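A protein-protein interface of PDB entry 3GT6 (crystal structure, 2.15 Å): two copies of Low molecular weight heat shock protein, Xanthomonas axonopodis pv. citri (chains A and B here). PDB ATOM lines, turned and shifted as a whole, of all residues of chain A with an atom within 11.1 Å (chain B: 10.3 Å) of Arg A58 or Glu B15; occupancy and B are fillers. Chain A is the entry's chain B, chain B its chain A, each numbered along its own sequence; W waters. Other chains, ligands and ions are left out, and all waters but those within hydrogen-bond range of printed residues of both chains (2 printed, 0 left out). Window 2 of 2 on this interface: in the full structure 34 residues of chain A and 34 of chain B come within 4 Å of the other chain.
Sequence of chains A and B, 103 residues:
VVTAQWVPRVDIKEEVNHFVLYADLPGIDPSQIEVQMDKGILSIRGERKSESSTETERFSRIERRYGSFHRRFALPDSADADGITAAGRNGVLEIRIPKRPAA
Ser A53 touches none of the printed residues of chain B.
No residue of chain B comes within 4 Å of Glu A57.
Arg A58 touches just these residues of chain B: Lys B13, Glu B14 and Glu B15.
Of chain B, only Asp B11, Ile B12, Lys B13 and Tyr B22 come within 4 Å of Phe A59.
Printed residues of chain B within 4 Å of Ser A60: Ile B12.
Printed residues of chain A within 4 Å of Asp B11: Ser A50, Ser A52, Phe A59, Arg A61 and Ile A62.
Lys B13 touches just these residues of chain A: Arg A58 and Phe A59.
Glu B15 touches just these residues of chain A: Glu A55 (3.8 Å) and Arg A58 (3.5 Å).
No residue of chain A comes within 4 Å of Val B16.
No residue of chain A comes within 4 Å of Asn B17.
His B18 touches none of the printed residues of chain A.
Of the printed residues of chain A, Tyr B22 touches Glu A51 (3.3 Å) and Phe A59 (3.9 Å).
Ile B97 touches none of the printed residues of chain A.
Of the 13 printed residues of chain A, 9 touch a printed residue of chain B.
Hydrophobic or aromatic side chains of chain A within 4 Å of the printed part of chain B: Phe A59.
Along chain A the printed residues that touch a printed residue of chain B span positions 50 to 62.
Printed residues of chain B that touch a printed residue of chain A: Asp B11, Ile B12, Lys B13, Glu B14, Glu B15 and Tyr B22.
Hydrophobic or aromatic side chains of chain B that line the printed part of chain A: Ile B12 and Tyr B22.
The guanidinium group of Arg A58 is in salt-bridge range of the side-chain carboxylate of Glu B15, 3.8 Å away.
The backbone NH (N) of Ile B12 is in hydrogen-bond range of the backbone carbonyl oxygen (O) of Arg A61 (2.8 Å).
N of Glu B14 is in hydrogen-bond range of O of Arg A58, 2.8 Å away.
The backbone NH of Ser A60 is in hydrogen-bond range of the backbone carbonyl oxygen of Ile B12, at 2.8 Å.
Water W1 lies within hydrogen-bond range of the side-chain hydroxyl of Ser A50, the side-chain carboxylate of Asp B11 and the side-chain hydroxyl of Ser A52.
Water W2 bridges the side-chain carboxylate of Glu B94 (2.6 Å) and the side-chain carboxylate of Glu A51 (2.9 Å).
The backbone carbonyl oxygen of Val B20 sits at hydrogen-bond distance from the backbone NH of Lys B13 (2.8 Å).
The side-chain hydroxyl of Ser A50 sits close to the backbone NH of Ser A52, at 3.1 Å.
The backbone carbonyl oxygen of Asp B11 lies within hydrogen-bond range of the backbone NH of Tyr B22.
The side-chain hydroxyl of Ser A53 is in hydrogen-bond range of the backbone carbonyl oxygen of Ser A50, 3.0 Å away.
The side-chain carboxylate (OE2) of Glu B14 lies within salt-bridge range of the side-chain amino group (NZ) of Lys B99.
The backbone carbonyl oxygen (O) of Glu B15 is in hydrogen-bond range of the side-chain amino group (NZ) of Lys B99, 3.0 Å away.
No position is printed for both chains.
Of the 15 pairs that touch across the chains among the printed residues, none has its exchanged pair printed and touching as well.
Among the printed residues, merely in contact across the chains: Ser A50 with Asp B11, Glu A51 with Tyr B22, Ser A52 with Asp B11, Glu A55 with Glu B15, Arg A58 with Lys B13, Phe A59 with Asp B11, Phe A59 with Ile B12, Phe A59 with Lys B13, Phe A59 with Tyr B22, Arg A61 with Asp B11 and Ile A62 with Asp B11.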
ATOM      1  N   SER A  50      -1.765  -4.542  16.886  1.00  0.00           N
ATOM      2  CA  SER A  50      -2.380  -4.158  15.613  1.00  0.00           C
ATOM      3  C   SER A  50      -2.921  -2.768  15.735  1.00  0.00           C
ATOM      4  O   SER A  50      -3.468  -2.381  16.771  1.00  0.00           O
ATOM      5  CB  SER A  50      -3.500  -5.133  15.232  1.00  0.00           C
ATOM      6  OG  SER A  50      -4.135  -4.689  14.069  1.00  0.00           O
ATOM      7  N   GLU A  51      -2.785  -2.021  14.650  1.00  0.00           N
ATOM      8  CA  GLU A  51      -3.329  -0.706  14.583  1.00  0.00           C
ATOM      9  C   GLU A  51      -4.844  -0.750  14.885  1.00  0.00           C
ATOM     10  O   GLU A  51      -5.414   0.227  15.383  1.00  0.00           O
ATOM     11  CB  GLU A  51      -3.007  -0.090  13.220  1.00  0.00           C
ATOM     12  CG  GLU A  51      -1.458  -0.065  12.922  1.00  0.00           C
ATOM     13  CD  GLU A  51      -0.843  -1.418  12.280  1.00  0.00           C
ATOM     14  OE1 GLU A  51      -1.459  -2.529  12.381  1.00  0.00           O
ATOM     15  OE2 GLU A  51       0.293  -1.358  11.667  1.00  0.00           O
ATOM     16  N   SER A  52      -5.479  -1.904  14.646  1.00  0.00           N
ATOM     17  CA  SER A  52      -6.904  -1.943  14.817  1.00  0.00           C
ATOM     18  C   SER A  52      -7.449  -1.812  16.255  1.00  0.00           C
ATOM     19  O   SER A  52      -8.678  -1.651  16.428  1.00  0.00           O
ATOM     20  CB  SER A  52      -7.523  -3.162  14.136  1.00  0.00           C
ATOM     21  OG  SER A  52      -7.245  -4.324  14.864  1.00  0.00           O
ATOM     22  N   SER A  53      -6.592  -1.951  17.272  1.00  0.00           N
ATOM     23  CA  SER A  53      -7.070  -1.899  18.686  1.00  0.00           C
ATOM     24  C   SER A  53      -7.013  -0.463  19.143  1.00  0.00           C
ATOM     25  O   SER A  53      -7.534  -0.119  20.207  1.00  0.00           O
ATOM     26  CB  SER A  53      -6.215  -2.802  19.590  1.00  0.00           C
ATOM     27  OG  SER A  53      -4.854  -2.455  19.392  1.00  0.00           O
ATOM     28  N   THR A  54      -6.403   0.394  18.319  1.00  0.00           N
ATOM     29  CA  THR A  54      -6.491   1.856  18.520  1.00  0.00           C
ATOM     30  C   THR A  54      -7.550   2.454  17.610  1.00  0.00           C
ATOM     31  O   THR A  54      -7.500   2.210  16.411  1.00  0.00           O
ATOM     32  CB  THR A  54      -5.141   2.507  18.192  1.00  0.00           C
ATOM     33  OG1 THR A  54      -4.227   2.053  19.176  1.00  0.00           O
ATOM     34  CG2 THR A  54      -5.186   4.020  18.271  1.00  0.00           C
ATOM     35  N   GLU A  55      -8.472   3.249  18.163  1.00  0.00           N
ATOM     36  CA  GLU A  55      -9.536   3.931  17.367  1.00  0.00           C
ATOM     37  C   GLU A  55     -10.212   2.861  16.559  1.00  0.00           C
ATOM     38  O   GLU A  55     -10.315   3.006  15.333  1.00  0.00           O
ATOM     39  CB  GLU A  55      -8.999   4.956  16.340  1.00  0.00           C
ATOM     40  CG  GLU A  55      -7.884   6.005  16.739  1.00  0.00           C
ATOM     41  CD  GLU A  55      -8.279   6.978  17.839  1.00  0.00           C
ATOM     42  OE1 GLU A  55      -9.471   7.011  18.224  1.00  0.00           O
ATOM     43  OE2 GLU A  55      -7.375   7.708  18.325  1.00  0.00           O
ATOM     44  N   THR A  56     -10.561   1.752  17.210  1.00  0.00           N
ATOM     45  CA  THR A  56     -11.201   0.633  16.578  1.00  0.00           C
ATOM     46  C   THR A  56     -12.442   1.064  15.785  1.00  0.00           C
ATOM     47  O   THR A  56     -12.672   0.576  14.674  1.00  0.00           O
ATOM     48  CB  THR A  56     -11.510  -0.465  17.602  1.00  0.00           C
ATOM     49  OG1 THR A  56     -10.271  -0.766  18.312  1.00  0.00           O
ATOM     50  CG2 THR A  56     -12.002  -1.748  16.883  1.00  0.00           C
ATOM     51  N   GLU A  57     -13.176   2.037  16.313  1.00  0.00           N
ATOM     52  CA  GLU A  57     -14.450   2.420  15.726  1.00  0.00           C
ATOM     53  C   GLU A  57     -14.214   3.080  14.338  1.00  0.00           C
ATOM     54  O   GLU A  57     -15.164   3.260  13.586  1.00  0.00           O
ATOM     55  CB  GLU A  57     -15.199   3.375  16.694  1.00  0.00           C
ATOM     56  CG  GLU A  57     -14.409   4.700  16.990  1.00  0.00           C
ATOM     57  CD  GLU A  57     -13.167   4.553  17.989  1.00  0.00           C
ATOM     58  OE1 GLU A  57     -13.065   3.514  18.736  1.00  0.00           O
ATOM     59  OE2 GLU A  57     -12.313   5.518  18.008  1.00  0.00           O
ATOM     60  N   ARG A  58     -12.950   3.405  14.006  1.00  0.00           N
ATOM     61  CA  ARG A  58     -12.623   4.092  12.761  1.00  0.00           C
ATOM     62  C   ARG A  58     -12.404   3.074  11.657  1.00  0.00           C
ATOM     63  O   ARG A  58     -12.268   3.418  10.525  1.00  0.00           O
ATOM     64  CB  ARG A  58     -11.385   4.978  12.946  1.00  0.00           C
ATOM     65  CG  ARG A  58     -11.701   6.148  13.951  1.00  0.00           C
ATOM     66  CD  ARG A  58     -10.911   7.381  13.644  1.00  0.00           C
ATOM     67  NE  ARG A  58     -11.579   8.610  14.052  1.00  0.00           N
ATOM     68  CZ  ARG A  58     -11.286   9.276  15.165  1.00  0.00           C
ATOM     69  NH1 ARG A  58     -11.948  10.391  15.442  1.00  0.00           N
ATOM     70  NH2 ARG A  58     -10.340   8.834  15.994  1.00  0.00           N
ATOM     71  N   PHE A  59     -12.370   1.803  12.018  1.00  0.00           N
ATOM     72  CA  PHE A  59     -12.034   0.789  11.020  1.00  0.00           C
ATOM     73  C   PHE A  59     -13.296   0.368  10.407  1.00  0.00           C
ATOM     74  O   PHE A  59     -14.315   0.156  11.087  1.00  0.00           O
ATOM     75  CB  PHE A  59     -11.407  -0.397  11.656  1.00  0.00           C
ATOM     76  CG  PHE A  59      -9.976  -0.169  12.002  1.00  0.00           C
ATOM     77  CD1 PHE A  59      -8.970  -0.797  11.261  1.00  0.00           C
ATOM     78  CD2 PHE A  59      -9.613   0.687  13.035  1.00  0.00           C
ATOM     79  CE1 PHE A  59      -7.605  -0.587  11.544  1.00  0.00           C
ATOM     80  CE2 PHE A  59      -8.235   0.903  13.310  1.00  0.00           C
ATOM     81  CZ  PHE A  59      -7.252   0.266  12.570  1.00  0.00           C
ATOM     82  N   SER A  60     -13.226   0.241   9.115  1.00  0.00           N
ATOM     83  CA  SER A  60     -14.404  -0.130   8.345  1.00  0.00           C
ATOM     84  C   SER A  60     -14.179  -1.571   8.022  1.00  0.00           C
ATOM     85  O   SER A  60     -15.047  -2.231   7.483  1.00  0.00           O
ATOM     86  CB  SER A  60     -14.347   0.739   7.084  1.00  0.00           C
ATOM     87  OG  SER A  60     -13.307   0.247   6.242  1.00  0.00           O
ATOM     88  N   ARG A  61     -12.982  -2.098   8.310  1.00  0.00           N
ATOM     89  CA  ARG A  61     -12.785  -3.530   8.170  1.00  0.00           C
ATOM     90  C   ARG A  61     -11.639  -3.970   9.051  1.00  0.00           C
ATOM     91  O   ARG A  61     -10.551  -3.357   9.057  1.00  0.00           O
ATOM     92  CB  ARG A  61     -12.416  -3.827   6.716  1.00  0.00           C
ATOM     93  CG  ARG A  61     -12.083  -5.265   6.404  1.00  0.00           C
ATOM     94  CD  ARG A  61     -11.350  -5.288   5.027  1.00  0.00           C
ATOM     95  NE  ARG A  61     -10.972  -6.658   4.775  1.00  0.00           N
ATOM     96  CZ  ARG A  61     -11.858  -7.580   4.409  1.00  0.00           C
ATOM     97  NH1 ARG A  61     -11.503  -8.858   4.215  1.00  0.00           N
ATOM     98  NH2 ARG A  61     -13.100  -7.191   4.178  1.00  0.00           N
ATOM     99  N   ILE A  62     -11.843  -5.052   9.784  1.00  0.00           N
ATOM    100  CA  ILE A  62     -10.760  -5.564  10.595  1.00  0.00           C
ATOM    101  C   ILE A  62     -10.752  -7.051  10.437  1.00  0.00           C
ATOM    102  O   ILE A  62     -11.762  -7.702  10.655  1.00  0.00           O
ATOM    103  CB  ILE A  62     -11.059  -5.311  12.089  1.00  0.00           C
ATOM    104  CG1 ILE A  62     -11.083  -3.834  12.354  1.00  0.00           C
ATOM    105  CG2 ILE A  62      -9.977  -6.022  13.047  1.00  0.00           C
ATOM    106  CD1 ILE A  62     -11.575  -3.493  13.784  1.00  0.00           C
ATOM    107  N   ASP B  11      -6.786  -4.681   7.193  1.00  0.00           N
ATOM    108  CA  ASP B  11      -7.633  -3.851   8.006  1.00  0.00           C
ATOM    109  C   ASP B  11      -7.724  -2.535   7.314  1.00  0.00           C
ATOM    110  O   ASP B  11      -6.761  -2.103   6.645  1.00  0.00           O
ATOM    111  CB  ASP B  11      -6.966  -3.590   9.345  1.00  0.00           C
ATOM    112  CG  ASP B  11      -6.822  -4.822  10.157  1.00  0.00           C
ATOM    113  OD1 ASP B  11      -7.511  -5.816   9.832  1.00  0.00           O
ATOM    114  OD2 ASP B  11      -5.962  -4.814  11.067  1.00  0.00           O
ATOM    115  N   ILE B  12      -8.880  -1.885   7.413  1.00  0.00           N
ATOM    116  CA  ILE B  12      -8.981  -0.616   6.752  1.00  0.00           C
ATOM    117  C   ILE B  12      -9.545   0.338   7.796  1.00  0.00           C
ATOM    118  O   ILE B  12     -10.510   0.018   8.471  1.00  0.00           O
ATOM    119  CB  ILE B  12      -9.913  -0.712   5.589  1.00  0.00           C
ATOM    120  CG1 ILE B  12      -9.371  -1.725   4.587  1.00  0.00           C
ATOM    121  CG2 ILE B  12     -10.084   0.721   4.877  1.00  0.00           C
ATOM    122  CD1 ILE B  12     -10.415  -1.987   3.466  1.00  0.00           C
ATOM    123  N   LYS B  13      -8.969   1.518   7.883  1.00  0.00           N
ATOM    124  CA  LYS B  13      -9.358   2.491   8.844  1.00  0.00           C
ATOM    125  C   LYS B  13      -9.631   3.784   8.088  1.00  0.00           C
ATOM    126  O   LYS B  13      -8.927   4.135   7.133  1.00  0.00           O
ATOM    127  CB  LYS B  13      -8.160   2.677   9.777  1.00  0.00           C
ATOM    128  CG  LYS B  13      -8.226   3.831  10.712  1.00  0.00           C
ATOM    129  CD  LYS B  13      -7.025   3.991  11.661  1.00  0.00           C
ATOM    130  CE  LYS B  13      -5.823   4.570  10.959  1.00  0.00           C
ATOM    131  NZ  LYS B  13      -4.762   4.923  11.937  1.00  0.00           N
ATOM    132  N   GLU B  14     -10.665   4.499   8.500  1.00  0.00           N
ATOM    133  CA  GLU B  14     -10.910   5.809   7.956  1.00  0.00           C
ATOM    134  C   GLU B  14     -10.691   6.769   9.086  1.00  0.00           C
ATOM    135  O   GLU B  14     -11.379   6.722  10.094  1.00  0.00           O
ATOM    136  CB  GLU B  14     -12.365   5.928   7.519  1.00  0.00           C
ATOM    137  CG  GLU B  14     -12.593   7.358   7.004  1.00  0.00           C
ATOM    138  CD  GLU B  14     -13.973   7.581   6.433  1.00  0.00           C
ATOM    139  OE1 GLU B  14     -14.668   6.606   6.130  1.00  0.00           O
ATOM    140  OE2 GLU B  14     -14.346   8.744   6.274  1.00  0.00           O
ATOM    141  N   GLU B  15      -9.689   7.607   8.951  1.00  0.00           N
ATOM    142  CA  GLU B  15      -9.428   8.619   9.940  1.00  0.00           C
ATOM    143  C   GLU B  15     -10.112   9.895   9.464  1.00  0.00           C
ATOM    144  O   GLU B  15     -10.752   9.925   8.364  1.00  0.00           O
ATOM    145  CB  GLU B  15      -7.933   8.851  10.069  1.00  0.00           C
ATOM    146  CG  GLU B  15      -7.253   7.822  10.901  1.00  0.00           C
ATOM    147  CD  GLU B  15      -7.603   8.032  12.350  1.00  0.00           C
ATOM    148  OE1 GLU B  15      -8.078   9.151  12.670  1.00  0.00           O
ATOM    149  OE2 GLU B  15      -7.411   7.095  13.149  1.00  0.00           O
ATOM    150  N   VAL B  16      -9.952  10.950  10.258  1.00  0.00           N
ATOM    151  CA  VAL B  16     -10.588  12.223   9.940  1.00  0.00           C
ATOM    152  C   VAL B  16     -10.140  12.633   8.583  1.00  0.00           C
ATOM    153  O   VAL B  16     -10.973  12.999   7.744  1.00  0.00           O
ATOM    154  CB  VAL B  16     -10.266  13.384  10.962  1.00  0.00           C
ATOM    155  CG1 VAL B  16     -11.074  14.660  10.575  1.00  0.00           C
ATOM    156  CG2 VAL B  16     -10.619  12.985  12.376  1.00  0.00           C
ATOM    157  N   ASN B  17      -8.837  12.554   8.310  1.00  0.00           N
ATOM    158  CA  ASN B  17      -8.407  13.140   7.041  1.00  0.00           C
ATOM    159  C   ASN B  17      -7.687  12.156   6.123  1.00  0.00           C
ATOM    160  O   ASN B  17      -7.125  12.545   5.102  1.00  0.00           O
ATOM    161  CB  ASN B  17      -7.574  14.406   7.313  1.00  0.00           C
ATOM    162  CG  ASN B  17      -6.331  14.086   8.125  1.00  0.00           C
ATOM    163  OD1 ASN B  17      -5.932  12.895   8.228  1.00  0.00           O
ATOM    164  ND2 ASN B  17      -5.715  15.101   8.724  1.00  0.00           N
ATOM    165  N   HIS B  18      -7.726  10.868   6.460  1.00  0.00           N
ATOM    166  CA  HIS B  18      -7.057   9.935   5.598  1.00  0.00           C
ATOM    167  C   HIS B  18      -7.575   8.541   5.829  1.00  0.00           C
ATOM    168  O   HIS B  18      -8.249   8.266   6.827  1.00  0.00           O
ATOM    169  CB  HIS B  18      -5.512  10.035   5.812  1.00  0.00           C
ATOM    170  CG  HIS B  18      -5.064   9.545   7.150  1.00  0.00           C
ATOM    171  ND1 HIS B  18      -5.128  10.314   8.292  1.00  0.00           N
ATOM    172  CD2 HIS B  18      -4.532   8.353   7.531  1.00  0.00           C
ATOM    173  CE1 HIS B  18      -4.665   9.624   9.319  1.00  0.00           C
ATOM    174  NE2 HIS B  18      -4.277   8.441   8.876  1.00  0.00           N
ATOM    175  N   PHE B  19      -7.267   7.660   4.893  1.00  0.00           N
ATOM    176  CA  PHE B  19      -7.523   6.278   5.118  1.00  0.00           C
ATOM    177  C   PHE B  19      -6.201   5.608   5.292  1.00  0.00           C
ATOM    178  O   PHE B  19      -5.195   6.046   4.750  1.00  0.00           O
ATOM    179  CB  PHE B  19      -8.228   5.642   3.922  1.00  0.00           C
ATOM    180  CG  PHE B  19      -9.592   6.168   3.684  1.00  0.00           C
ATOM    181  CD1 PHE B  19     -10.707   5.451   4.149  1.00  0.00           C
ATOM    182  CD2 PHE B  19      -9.784   7.386   2.993  1.00  0.00           C
ATOM    183  CE1 PHE B  19     -12.021   5.934   3.899  1.00  0.00           C
ATOM    184  CE2 PHE B  19     -11.053   7.864   2.752  1.00  0.00           C
ATOM    185  CZ  PHE B  19     -12.205   7.137   3.211  1.00  0.00           C
ATOM    186  N   VAL B  20      -6.219   4.491   6.006  1.00  0.00           N
ATOM    187  CA  VAL B  20      -5.068   3.616   6.064  1.00  0.00           C
ATOM    188  C   VAL B  20      -5.585   2.207   5.864  1.00  0.00           C
ATOM    189  O   VAL B  20      -6.576   1.814   6.501  1.00  0.00           O
ATOM    190  CB  VAL B  20      -4.416   3.623   7.423  1.00  0.00           C
ATOM    191  CG1 VAL B  20      -3.052   2.960   7.272  1.00  0.00           C
ATOM    192  CG2 VAL B  20      -4.136   5.028   7.875  1.00  0.00           C
ATOM    193  N   LEU B  21      -4.917   1.476   4.990  1.00  0.00           N
ATOM    194  CA  LEU B  21      -5.123   0.038   4.855  1.00  0.00           C
ATOM    195  C   LEU B  21      -3.857  -0.589   5.304  1.00  0.00           C
ATOM    196  O   LEU B  21      -2.766  -0.144   4.995  1.00  0.00           O
ATOM    197  CB  LEU B  21      -5.442  -0.409   3.418  1.00  0.00           C
ATOM    198  CG  LEU B  21      -6.644   0.194   2.728  1.00  0.00           C
ATOM    199  CD1 LEU B  21      -6.283   1.594   2.222  1.00  0.00           C
ATOM    200  CD2 LEU B  21      -7.083  -0.686   1.568  1.00  0.00           C
ATOM    201  N   TYR B  22      -3.998  -1.612   6.108  1.00  0.00           N
ATOM    202  CA  TYR B  22      -2.837  -2.400   6.530  1.00  0.00           C
ATOM    203  C   TYR B  22      -3.049  -3.802   5.990  1.00  0.00           C
ATOM    204  O   TYR B  22      -4.062  -4.408   6.331  1.00  0.00           O
ATOM    205  CB  TYR B  22      -2.889  -2.540   8.053  1.00  0.00           C
ATOM    206  CG  TYR B  22      -2.988  -1.201   8.755  1.00  0.00           C
ATOM    207  CD1 TYR B  22      -1.842  -0.506   9.111  1.00  0.00           C
ATOM    208  CD2 TYR B  22      -4.237  -0.653   9.098  1.00  0.00           C
ATOM    209  CE1 TYR B  22      -1.899   0.719   9.758  1.00  0.00           C
ATOM    210  CE2 TYR B  22      -4.316   0.572   9.761  1.00  0.00           C
ATOM    211  CZ  TYR B  22      -3.134   1.253  10.071  1.00  0.00           C
ATOM    212  OH  TYR B  22      -3.169   2.449  10.715  1.00  0.00           O
ATOM    213  N   LEU B  75     -13.520   1.971  -1.727  1.00  0.00           N
ATOM    214  CA  LEU B  75     -13.319   2.982  -0.737  1.00  0.00           C
ATOM    215  C   LEU B  75     -14.305   4.145  -1.004  1.00  0.00           C
ATOM    216  O   LEU B  75     -14.776   4.306  -2.120  1.00  0.00           O
ATOM    217  CB  LEU B  75     -11.906   3.528  -0.798  1.00  0.00           C
ATOM    218  CG  LEU B  75     -10.854   2.513  -0.299  1.00  0.00           C
ATOM    219  CD1 LEU B  75      -9.557   3.269  -0.184  1.00  0.00           C
ATOM    220  CD2 LEU B  75     -11.328   2.073   1.040  1.00  0.00           C
ATOM    221  N   PRO B  76     -14.605   4.942   0.011  1.00  0.00           N
ATOM    222  CA  PRO B  76     -15.521   6.095  -0.232  1.00  0.00           C
ATOM    223  C   PRO B  76     -14.907   7.090  -1.210  1.00  0.00           C
ATOM    224  O   PRO B  76     -13.670   7.092  -1.392  1.00  0.00           O
ATOM    225  CB  PRO B  76     -15.660   6.754   1.160  1.00  0.00           C
ATOM    226  CG  PRO B  76     -15.297   5.631   2.143  1.00  0.00           C
ATOM    227  CD  PRO B  76     -14.167   4.850   1.413  1.00  0.00           C
ATOM    228  N   SER B  78     -14.357  10.098  -0.871  1.00  0.00           N
ATOM    229  CA  SER B  78     -13.449  11.023  -0.241  1.00  0.00           C
ATOM    230  C   SER B  78     -11.995  10.609  -0.339  1.00  0.00           C
ATOM    231  O   SER B  78     -11.115  11.465  -0.080  1.00  0.00           O
ATOM    232  CB  SER B  78     -13.782  11.194   1.230  1.00  0.00           C
ATOM    233  OG  SER B  78     -13.594   9.958   1.932  1.00  0.00           O
ATOM    234  N   ALA B  79     -11.734   9.322  -0.666  1.00  0.00           N
ATOM    235  CA  ALA B  79     -10.359   8.800  -0.795  1.00  0.00           C
ATOM    236  C   ALA B  79      -9.737   9.465  -2.019  1.00  0.00           C
ATOM    237  O   ALA B  79     -10.212   9.262  -3.138  1.00  0.00           O
ATOM    238  CB  ALA B  79     -10.347   7.315  -0.952  1.00  0.00           C
ATOM    239  N   GLU B  94       1.398  -0.804   4.445  1.00  0.00           N
ATOM    240  CA  GLU B  94       0.573   0.197   4.974  1.00  0.00           C
ATOM    241  C   GLU B  94       0.307   1.183   3.870  1.00  0.00           C
ATOM    242  O   GLU B  94       1.225   1.799   3.321  1.00  0.00           O
ATOM    243  CB  GLU B  94       1.297   0.897   6.132  1.00  0.00           C
ATOM    244  CG  GLU B  94       0.379   1.873   6.723  1.00  0.00           C
ATOM    245  CD  GLU B  94       0.941   2.546   7.955  1.00  0.00           C
ATOM    246  OE1 GLU B  94       1.493   1.853   8.834  1.00  0.00           O
ATOM    247  OE2 GLU B  94       0.818   3.764   7.999  1.00  0.00           O
ATOM    248  N   ILE B  95      -0.956   1.296   3.486  1.00  0.00           N
ATOM    249  CA  ILE B  95      -1.314   2.148   2.394  1.00  0.00           C
ATOM    250  C   ILE B  95      -2.090   3.320   2.982  1.00  0.00           C
ATOM    251  O   ILE B  95      -3.078   3.120   3.651  1.00  0.00           O
ATOM    252  CB  ILE B  95      -2.257   1.414   1.475  1.00  0.00           C
ATOM    253  CG1 ILE B  95      -1.556   0.161   0.972  1.00  0.00           C
ATOM    254  CG2 ILE B  95      -2.768   2.357   0.391  1.00  0.00           C
ATOM    255  CD1 ILE B  95      -2.497  -0.829   0.303  1.00  0.00           C
ATOM    256  N   ARG B  96      -1.641   4.531   2.708  1.00  0.00           N
ATOM    257  CA  ARG B  96      -2.205   5.707   3.291  1.00  0.00           C
ATOM    258  C   ARG B  96      -2.767   6.528   2.184  1.00  0.00           C
ATOM    259  O   ARG B  96      -2.134   6.687   1.149  1.00  0.00           O
ATOM    260  CB  ARG B  96      -1.107   6.452   4.036  1.00  0.00           C
ATOM    261  CG  ARG B  96      -0.487   5.625   5.171  1.00  0.00           C
ATOM    262  CD  ARG B  96       0.661   6.414   5.846  1.00  0.00           C
ATOM    263  NE  ARG B  96       0.094   7.492   6.690  1.00  0.00           N
ATOM    264  CZ  ARG B  96      -0.487   7.340   7.897  1.00  0.00           C
ATOM    265  NH1 ARG B  96      -0.534   6.169   8.488  1.00  0.00           N
ATOM    266  NH2 ARG B  96      -0.970   8.409   8.551  1.00  0.00           N
ATOM    267  N   ILE B  97      -4.000   6.977   2.352  1.00  0.00           N
ATOM    268  CA  ILE B  97      -4.681   7.702   1.307  1.00  0.00           C
ATOM    269  C   ILE B  97      -5.355   8.899   1.979  1.00  0.00           C
ATOM    270  O   ILE B  97      -6.253   8.742   2.775  1.00  0.00           O
ATOM    271  CB  ILE B  97      -5.719   6.882   0.686  1.00  0.00           C
ATOM    272  CG1 ILE B  97      -5.151   5.483   0.383  1.00  0.00           C
ATOM    273  CG2 ILE B  97      -6.165   7.589  -0.518  1.00  0.00           C
ATOM    274  CD1 ILE B  97      -6.128   4.550  -0.287  1.00  0.00           C
ATOM    275  N   PRO B  98      -4.900  10.106   1.685  1.00  0.00           N
ATOM    276  CA  PRO B  98      -5.601  11.265   2.241  1.00  0.00           C
ATOM    277  C   PRO B  98      -6.986  11.358   1.671  1.00  0.00           C
ATOM    278  O   PRO B  98      -7.290  10.829   0.605  1.00  0.00           O
ATOM    279  CB  PRO B  98      -4.815  12.449   1.730  1.00  0.00           C
ATOM    280  CG  PRO B  98      -3.932  11.964   0.647  1.00  0.00           C
ATOM    281  CD  PRO B  98      -3.967  10.460   0.608  1.00  0.00           C
ATOM    282  N   LYS B  99      -7.852  11.996   2.430  1.00  0.00           N
ATOM    283  CA  LYS B  99      -9.157  12.354   1.880  1.00  0.00           C
ATOM    284  C   LYS B  99      -9.074  13.652   1.109  1.00  0.00           C
ATOM    285  O   LYS B  99      -8.301  14.551   1.472  1.00  0.00           O
ATOM    286  CB  LYS B  99     -10.135  12.514   2.990  1.00  0.00           C
ATOM    287  CG  LYS B  99     -10.368  11.308   3.763  1.00  0.00           C
ATOM    288  CD  LYS B  99     -11.423  11.677   4.798  1.00  0.00           C
ATOM    289  CE  LYS B  99     -11.790  10.474   5.521  1.00  0.00           C
ATOM    290  NZ  LYS B  99     -12.838  10.833   6.443  1.00  0.00           N
ATOM    291  N   ARG B 100      -9.840  13.707   0.022  1.00  0.00           N
ATOM    292  CA  ARG B 100     -10.100  14.892  -0.782  1.00  0.00           C
ATOM    293  C   ARG B 100     -10.468  16.082   0.128  1.00  0.00           C
ATOM    294  O   ARG B 100     -11.086  15.906   1.201  1.00  0.00           O
ATOM    295  CB  ARG B 100     -11.234  14.606  -1.791  1.00  0.00           C
ATOM    296  CG  ARG B 100     -10.799  13.635  -2.928  1.00  0.00           C
ATOM    297  CD  ARG B 100     -11.867  13.177  -3.955  1.00  0.00           C
ATOM    298  NE  ARG B 100     -11.397  11.934  -4.607  1.00  0.00           N
ATOM    299  CZ  ARG B 100     -10.370  11.831  -5.497  1.00  0.00           C
ATOM    300  NH1 ARG B 100     -10.005  10.627  -5.991  1.00  0.00           N
ATOM    301  NH2 ARG B 100      -9.660  12.913  -5.887  1.00  0.00           N
HETATM  302  O   HOH W   1      -5.959  -6.124  13.316  1.00  0.00           O
HETATM  303  O   HOH W   2       1.559  -0.685   9.200  1.00  0.00           O
